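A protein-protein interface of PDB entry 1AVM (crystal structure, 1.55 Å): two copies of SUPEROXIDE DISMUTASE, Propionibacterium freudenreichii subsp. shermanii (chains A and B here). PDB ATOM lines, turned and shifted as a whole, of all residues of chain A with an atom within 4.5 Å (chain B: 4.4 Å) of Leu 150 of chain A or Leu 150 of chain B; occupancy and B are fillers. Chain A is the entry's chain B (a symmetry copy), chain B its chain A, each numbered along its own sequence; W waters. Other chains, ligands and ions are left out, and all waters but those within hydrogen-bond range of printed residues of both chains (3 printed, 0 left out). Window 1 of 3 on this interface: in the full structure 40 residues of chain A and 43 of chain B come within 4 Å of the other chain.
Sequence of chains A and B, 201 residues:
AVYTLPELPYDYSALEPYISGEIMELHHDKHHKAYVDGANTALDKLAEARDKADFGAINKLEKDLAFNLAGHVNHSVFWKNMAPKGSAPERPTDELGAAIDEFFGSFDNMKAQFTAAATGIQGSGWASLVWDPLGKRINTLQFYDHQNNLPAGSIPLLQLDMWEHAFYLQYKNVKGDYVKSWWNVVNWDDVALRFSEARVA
N of Asn 149 of chain A is in hydrogen-bond range of O of Gln 147 of chain B (2.9 Å). The backbone carbonyl oxygen (O) of Gln 147 of chain B sits at hydrogen-bond distance from the backbone NH (N) of Leu 150 of chain A. The side-chain amide oxygen of Asn 148 of chain B lies within hydrogen-bond range of the backbone NH of Asn 149 of chain A (2.9 Å). N of Asn 149 of chain B sits at hydrogen-bond distance from O of Gln 147 of chain A (2.9 Å). N of Asn 149 of chain B sits at hydrogen-bond distance from OD1 of Asn 148 of chain A, at 2.9 Å. The backbone NH (N) of Leu 150 of chain B sits at hydrogen-bond distance from the backbone carbonyl oxygen (O) of Gln 147 of chain A (3.0 Å).
Among the printed residues, pairs that only touch across the chains: Ala 66 of chain A with Asn 149 of chain B (3.4 Å), Ala 66 of chain A with Leu 150 of chain B (3.98 Å), Ala 66 of chain A with Pro 151 of chain B (3.96 Å), Gln 147 of chain A with Asn 148 of chain B (3.7 Å), Asn 148 of chain A with Gln 147 of chain B (3.7 Å), Asn 148 of chain A with Asn 148 of chain B (3.3 Å), Asn 149 of chain A with Ala 66 of chain B (3.4 Å), Leu 150 of chain A with Ala 66 of chain B (3.97 Å), Leu 150 of chain A with Leu 150 of chain B (3.6 Å), Leu 150 of chain A with Ala 152 of chain B (3.5 Å), Pro 151 of chain A with Ala 66 of chain B (3.97 Å) and Ala 152 of chain A with Leu 150 of chain B (3.5 Å).
Phe 143 of chain A touches none of the printed residues of chain B. Printed residues of chain B within 4 Å of Gln 147 of chain A: Asn 148, Asn 149 and Leu 150. Of the printed residues of chain B, Asn 149 of chain A touches Ala 66 (3.4 Å), Gln 147 (2.9 Å) and Asn 148 (2.9 Å). Printed residues of chain B within 4 Å of Leu 150 of chain A: Ala 66 (3.97 Å), Gln 147 (3.0 Å), Leu 150 (3.6 Å) and Ala 152 (3.5 Å). Phe 143 of chain B touches none of the printed residues of chain A. Printed residues of chain A within 4 Å of Asn 148 of chain B: Gln 147, Asn 148 and Asn 149. Of the printed residues of chain A, Asn 149 of chain B touches Ala 66, Gln 147 and Asn 148. Printed residues of chain A within 4 Å of Leu 150 of chain B: Ala 66 (3.98 Å), Gln 147 (3.0 Å), Leu 150 (3.6 Å) and Ala 152 (3.5 Å). The nearest residue of chain B that does not touch Leu 150 of chain A is Pro 151 of chain B (4.2 Å). The nearest printed residue of chain A that does not touch Leu 150 of chain B is Pro 151 of chain A (4.3 Å).
Of the 9 printed residues of chain B, 7 touch a printed residue of chain A. Printed residues of chain B that touch a printed residue of chain A: Ala 66, Gln 147, Asn 148, Asn 149, Leu 150, Pro 151 and Ala 152. Among the printed residues, 18 pairs touch across the chains.
Ala 66 of chain A touches Leu 150 of chain B, and with the chains exchanged Leu 150 of chain A touches Ala 66 of chain B. Ala 66 of chain A touches Pro 151 of chain B, and with the chains exchanged Pro 151 of chain A touches Ala 66 of chain B. Gln 147 of chain A touches Asn 148 of chain B, and with the chains exchanged Asn 148 of chain A touches Gln 147 of chain B. Asn 148 of chain A touches Asn 149 of chain B, and with the chains exchanged Asn 149 of chain A touches Asn 148 of chain B. Positions printed for both chains: 66, 141, 143, 147, 148, 149, 150, 151 and 152.
Water W1 lies within hydrogen-bond range of the side-chain amide nitrogen (ND2) of Asn 149 of chain B (2.8 Å), the side-chain amide oxygen (OE1) of Gln 147 of chain A (2.9 Å) and the side-chain amide oxygen (OD1) of Asn 148 of chain A (3.0 Å). Water W2 lies within hydrogen-bond range of ND2 of Asn 149 of chain A, OE1 of Gln 147 of chain B and OD1 of Asn 148 of chain B. Water W3 lies within hydrogen-bond range of O of Pro 151 of chain A (3.0 Å) and O of Pro 151 of chain B (3.1 Å).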
ATOM      1  N   ALA A  66       7.070   1.329  26.868  1.00  0.00           N
ATOM      2  CA  ALA A  66       7.896   2.257  26.101  1.00  0.00           C
ATOM      3  C   ALA A  66       9.353   1.809  26.016  1.00  0.00           C
ATOM      4  O   ALA A  66       9.925   1.760  24.932  1.00  0.00           O
ATOM      5  CB  ALA A  66       7.810   3.652  26.693  1.00  0.00           C
ATOM      6  N   LEU A 141      18.961  12.603  15.600  1.00  0.00           N
ATOM      7  CA  LEU A 141      18.447  12.678  16.961  1.00  0.00           C
ATOM      8  C   LEU A 141      19.388  11.877  17.843  1.00  0.00           C
ATOM      9  O   LEU A 141      20.105  10.995  17.365  1.00  0.00           O
ATOM     10  CB  LEU A 141      17.042  12.080  17.055  1.00  0.00           C
ATOM     11  CG  LEU A 141      15.890  12.810  16.361  1.00  0.00           C
ATOM     12  CD1 LEU A 141      14.615  12.005  16.550  1.00  0.00           C
ATOM     13  CD2 LEU A 141      15.724  14.214  16.931  1.00  0.00           C
ATOM     14  N   PHE A 143      18.984   9.650  21.032  1.00  0.00           N
ATOM     15  CA  PHE A 143      18.082   8.994  21.983  1.00  0.00           C
ATOM     16  C   PHE A 143      18.785   8.730  23.308  1.00  0.00           C
ATOM     17  O   PHE A 143      19.974   8.426  23.329  1.00  0.00           O
ATOM     18  CB  PHE A 143      17.609   7.625  21.468  1.00  0.00           C
ATOM     19  CG  PHE A 143      16.828   7.660  20.176  1.00  0.00           C
ATOM     20  CD1 PHE A 143      16.498   8.859  19.549  1.00  0.00           C
ATOM     21  CD2 PHE A 143      16.436   6.465  19.579  1.00  0.00           C
ATOM     22  CE1 PHE A 143      15.792   8.862  18.348  1.00  0.00           C
ATOM     23  CE2 PHE A 143      15.731   6.460  18.378  1.00  0.00           C
ATOM     24  CZ  PHE A 143      15.409   7.663  17.763  1.00  0.00           C
ATOM     25  N   GLN A 147      13.959   5.020  24.654  1.00  0.00           N
ATOM     26  CA  GLN A 147      12.717   5.744  24.475  1.00  0.00           C
ATOM     27  C   GLN A 147      12.635   7.222  24.840  1.00  0.00           C
ATOM     28  O   GLN A 147      11.533   7.766  24.942  1.00  0.00           O
ATOM     29  CB  GLN A 147      11.631   4.966  25.238  1.00  0.00           C
ATOM     30  CG  GLN A 147      11.612   5.131  26.785  1.00  0.00           C
ATOM     31  CD  GLN A 147      12.830   4.586  27.561  1.00  0.00           C
ATOM     32  OE1 GLN A 147      12.929   4.797  28.772  1.00  0.00           O
ATOM     33  NE2 GLN A 147      13.724   3.868  26.892  1.00  0.00           N
ATOM     34  N   ASN A 148      13.774   7.883  25.014  1.00  0.00           N
ATOM     35  CA  ASN A 148      13.748   9.296  25.384  1.00  0.00           C
ATOM     36  C   ASN A 148      14.470  10.201  24.398  1.00  0.00           C
ATOM     37  O   ASN A 148      15.345   9.756  23.655  1.00  0.00           O
ATOM     38  CB  ASN A 148      14.352   9.506  26.781  1.00  0.00           C
ATOM     39  CG  ASN A 148      13.633   8.714  27.863  1.00  0.00           C
ATOM     40  OD1 ASN A 148      12.413   8.560  27.838  1.00  0.00           O
ATOM     41  ND2 ASN A 148      14.398   8.207  28.825  1.00  0.00           N
ATOM     42  N   ASN A 149      14.074  11.475  24.407  1.00  0.00           N
ATOM     43  CA  ASN A 149      14.656  12.519  23.567  1.00  0.00           C
ATOM     44  C   ASN A 149      14.328  12.404  22.072  1.00  0.00           C
ATOM     45  O   ASN A 149      15.205  12.569  21.218  1.00  0.00           O
ATOM     46  CB  ASN A 149      16.176  12.584  23.790  1.00  0.00           C
ATOM     47  CG  ASN A 149      16.743  13.982  23.593  1.00  0.00           C
ATOM     48  OD1 ASN A 149      17.806  14.157  22.988  1.00  0.00           O
ATOM     49  ND2 ASN A 149      16.049  14.980  24.118  1.00  0.00           N
ATOM     50  N   LEU A 150      13.060  12.155  21.757  1.00  0.00           N
ATOM     51  CA  LEU A 150      12.630  12.041  20.362  1.00  0.00           C
ATOM     52  C   LEU A 150      11.164  12.439  20.182  1.00  0.00           C
ATOM     53  O   LEU A 150      10.340  12.217  21.070  1.00  0.00           O
ATOM     54  CB  LEU A 150      12.823  10.610  19.840  1.00  0.00           C
ATOM     55  CG  LEU A 150      11.865   9.524  20.346  1.00  0.00           C
ATOM     56  CD1 LEU A 150      11.813   8.366  19.360  1.00  0.00           C
ATOM     57  CD2 LEU A 150      12.278   9.047  21.721  1.00  0.00           C
ATOM     58  N   PRO A 151      10.832  13.070  19.039  1.00  0.00           N
ATOM     59  CA  PRO A 151       9.450  13.483  18.768  1.00  0.00           C
ATOM     60  C   PRO A 151       8.630  12.295  18.264  1.00  0.00           C
ATOM     61  O   PRO A 151       9.161  11.403  17.595  1.00  0.00           O
ATOM     62  CB  PRO A 151       9.608  14.518  17.643  1.00  0.00           C
ATOM     63  CG  PRO A 151      11.050  14.950  17.731  1.00  0.00           C
ATOM     64  CD  PRO A 151      11.747  13.664  18.051  1.00  0.00           C
ATOM     65  N   ALA A 152       7.342  12.282  18.585  1.00  0.00           N
ATOM     66  CA  ALA A 152       6.467  11.215  18.116  1.00  0.00           C
ATOM     67  C   ALA A 152       6.364  11.360  16.600  1.00  0.00           C
ATOM     68  O   ALA A 152       6.384  12.475  16.077  1.00  0.00           O
ATOM     69  CB  ALA A 152       5.092  11.344  18.748  1.00  0.00           C
ATOM     70  N   ALA B  66      14.724  17.934  19.921  1.00  0.00           N
ATOM     71  CA  ALA B  66      13.737  16.950  20.363  1.00  0.00           C
ATOM     72  C   ALA B  66      12.599  17.564  21.180  1.00  0.00           C
ATOM     73  O   ALA B  66      11.432  17.296  20.914  1.00  0.00           O
ATOM     74  CB  ALA B  66      14.413  15.840  21.159  1.00  0.00           C
ATOM     75  N   LEU B 141       0.250   5.432  25.374  1.00  0.00           N
ATOM     76  CA  LEU B 141       1.577   5.778  25.858  1.00  0.00           C
ATOM     77  C   LEU B 141       1.463   6.997  26.758  1.00  0.00           C
ATOM     78  O   LEU B 141       0.543   7.802  26.620  1.00  0.00           O
ATOM     79  CB  LEU B 141       2.518   6.085  24.693  1.00  0.00           C
ATOM     80  CG  LEU B 141       2.898   4.945  23.743  1.00  0.00           C
ATOM     81  CD1 LEU B 141       3.808   5.494  22.657  1.00  0.00           C
ATOM     82  CD2 LEU B 141       3.591   3.810  24.498  1.00  0.00           C
ATOM     83  N   PHE B 143       3.661  10.075  27.658  1.00  0.00           N
ATOM     84  CA  PHE B 143       4.843  10.884  27.365  1.00  0.00           C
ATOM     85  C   PHE B 143       5.242  11.706  28.587  1.00  0.00           C
ATOM     86  O   PHE B 143       4.379  12.158  29.348  1.00  0.00           O
ATOM     87  CB  PHE B 143       4.577  11.894  26.234  1.00  0.00           C
ATOM     88  CG  PHE B 143       4.224  11.286  24.900  1.00  0.00           C
ATOM     89  CD1 PHE B 143       4.247   9.910  24.694  1.00  0.00           C
ATOM     90  CD2 PHE B 143       3.855  12.116  23.844  1.00  0.00           C
ATOM     91  CE1 PHE B 143       3.910   9.372  23.453  1.00  0.00           C
ATOM     92  CE2 PHE B 143       3.517  11.588  22.601  1.00  0.00           C
ATOM     93  CZ  PHE B 143       3.543  10.210  22.406  1.00  0.00           C
ATOM     94  N   GLN B 147       8.967  14.848  24.646  1.00  0.00           N
ATOM     95  CA  GLN B 147       9.811  13.915  23.923  1.00  0.00           C
ATOM     96  C   GLN B 147      10.327  12.656  24.618  1.00  0.00           C
ATOM     97  O   GLN B 147      11.214  11.985  24.082  1.00  0.00           O
ATOM     98  CB  GLN B 147      11.003  14.708  23.374  1.00  0.00           C
ATOM     99  CG  GLN B 147      12.105  15.078  24.402  1.00  0.00           C
ATOM    100  CD  GLN B 147      11.723  16.129  25.463  1.00  0.00           C
ATOM    101  OE1 GLN B 147      12.499  16.379  26.391  1.00  0.00           O
ATOM    102  NE2 GLN B 147      10.570  16.768  25.308  1.00  0.00           N
ATOM    103  N   ASN B 148       9.785  12.321  25.784  1.00  0.00           N
ATOM    104  CA  ASN B 148      10.247  11.135  26.505  1.00  0.00           C
ATOM    105  C   ASN B 148       9.190  10.051  26.706  1.00  0.00           C
ATOM    106  O   ASN B 148       7.990  10.325  26.692  1.00  0.00           O
ATOM    107  CB  ASN B 148      10.810  11.529  27.876  1.00  0.00           C
ATOM    108  CG  ASN B 148      11.969  12.495  27.778  1.00  0.00           C
ATOM    109  OD1 ASN B 148      12.792  12.408  26.870  1.00  0.00           O
ATOM    110  ND2 ASN B 148      12.038  13.430  28.717  1.00  0.00           N
ATOM    111  N   ASN B 149       9.670   8.822  26.897  1.00  0.00           N
ATOM    112  CA  ASN B 149       8.835   7.652  27.152  1.00  0.00           C
ATOM    113  C   ASN B 149       7.980   7.173  25.967  1.00  0.00           C
ATOM    114  O   ASN B 149       6.792   6.883  26.127  1.00  0.00           O
ATOM    115  CB  ASN B 149       7.966   7.910  28.393  1.00  0.00           C
ATOM    116  CG  ASN B 149       7.633   6.642  29.157  1.00  0.00           C
ATOM    117  OD1 ASN B 149       6.500   6.457  29.605  1.00  0.00           O
ATOM    118  ND2 ASN B 149       8.624   5.777  29.338  1.00  0.00           N
ATOM    119  N   LEU B 150       8.598   7.060  24.793  1.00  0.00           N
ATOM    120  CA  LEU B 150       7.899   6.600  23.590  1.00  0.00           C
ATOM    121  C   LEU B 150       8.852   5.974  22.575  1.00  0.00           C
ATOM    122  O   LEU B 150      10.011   6.375  22.466  1.00  0.00           O
ATOM    123  CB  LEU B 150       7.143   7.753  22.912  1.00  0.00           C
ATOM    124  CG  LEU B 150       7.968   8.830  22.202  1.00  0.00           C
ATOM    125  CD1 LEU B 150       7.162   9.441  21.069  1.00  0.00           C
ATOM    126  CD2 LEU B 150       8.418   9.890  23.185  1.00  0.00           C
ATOM    127  N   PRO B 151       8.384   4.952  21.843  1.00  0.00           N
ATOM    128  CA  PRO B 151       9.207   4.279  20.833  1.00  0.00           C
ATOM    129  C   PRO B 151       9.251   5.091  19.539  1.00  0.00           C
ATOM    130  O   PRO B 151       8.309   5.823  19.220  1.00  0.00           O
ATOM    131  CB  PRO B 151       8.460   2.960  20.599  1.00  0.00           C
ATOM    132  CG  PRO B 151       7.652   2.769  21.855  1.00  0.00           C
ATOM    133  CD  PRO B 151       7.171   4.166  22.123  1.00  0.00           C
ATOM    134  N   ALA B 152      10.350   4.968  18.805  1.00  0.00           N
ATOM    135  CA  ALA B 152      10.494   5.660  17.530  1.00  0.00           C
ATOM    136  C   ALA B 152       9.493   5.017  16.579  1.00  0.00           C
ATOM    137  O   ALA B 152       9.231   3.816  16.671  1.00  0.00           O
ATOM    138  CB  ALA B 152      11.907   5.487  16.992  1.00  0.00           C
HETATM  139  O   HOH W   1      11.159   6.806  29.864  1.00  0.00           O
HETATM  140  O   HOH W   2      14.768  14.550  26.593  1.00  0.00           O
HETATM  141  O   HOH W   3       8.485   8.440  17.556  1.00  0.00           O
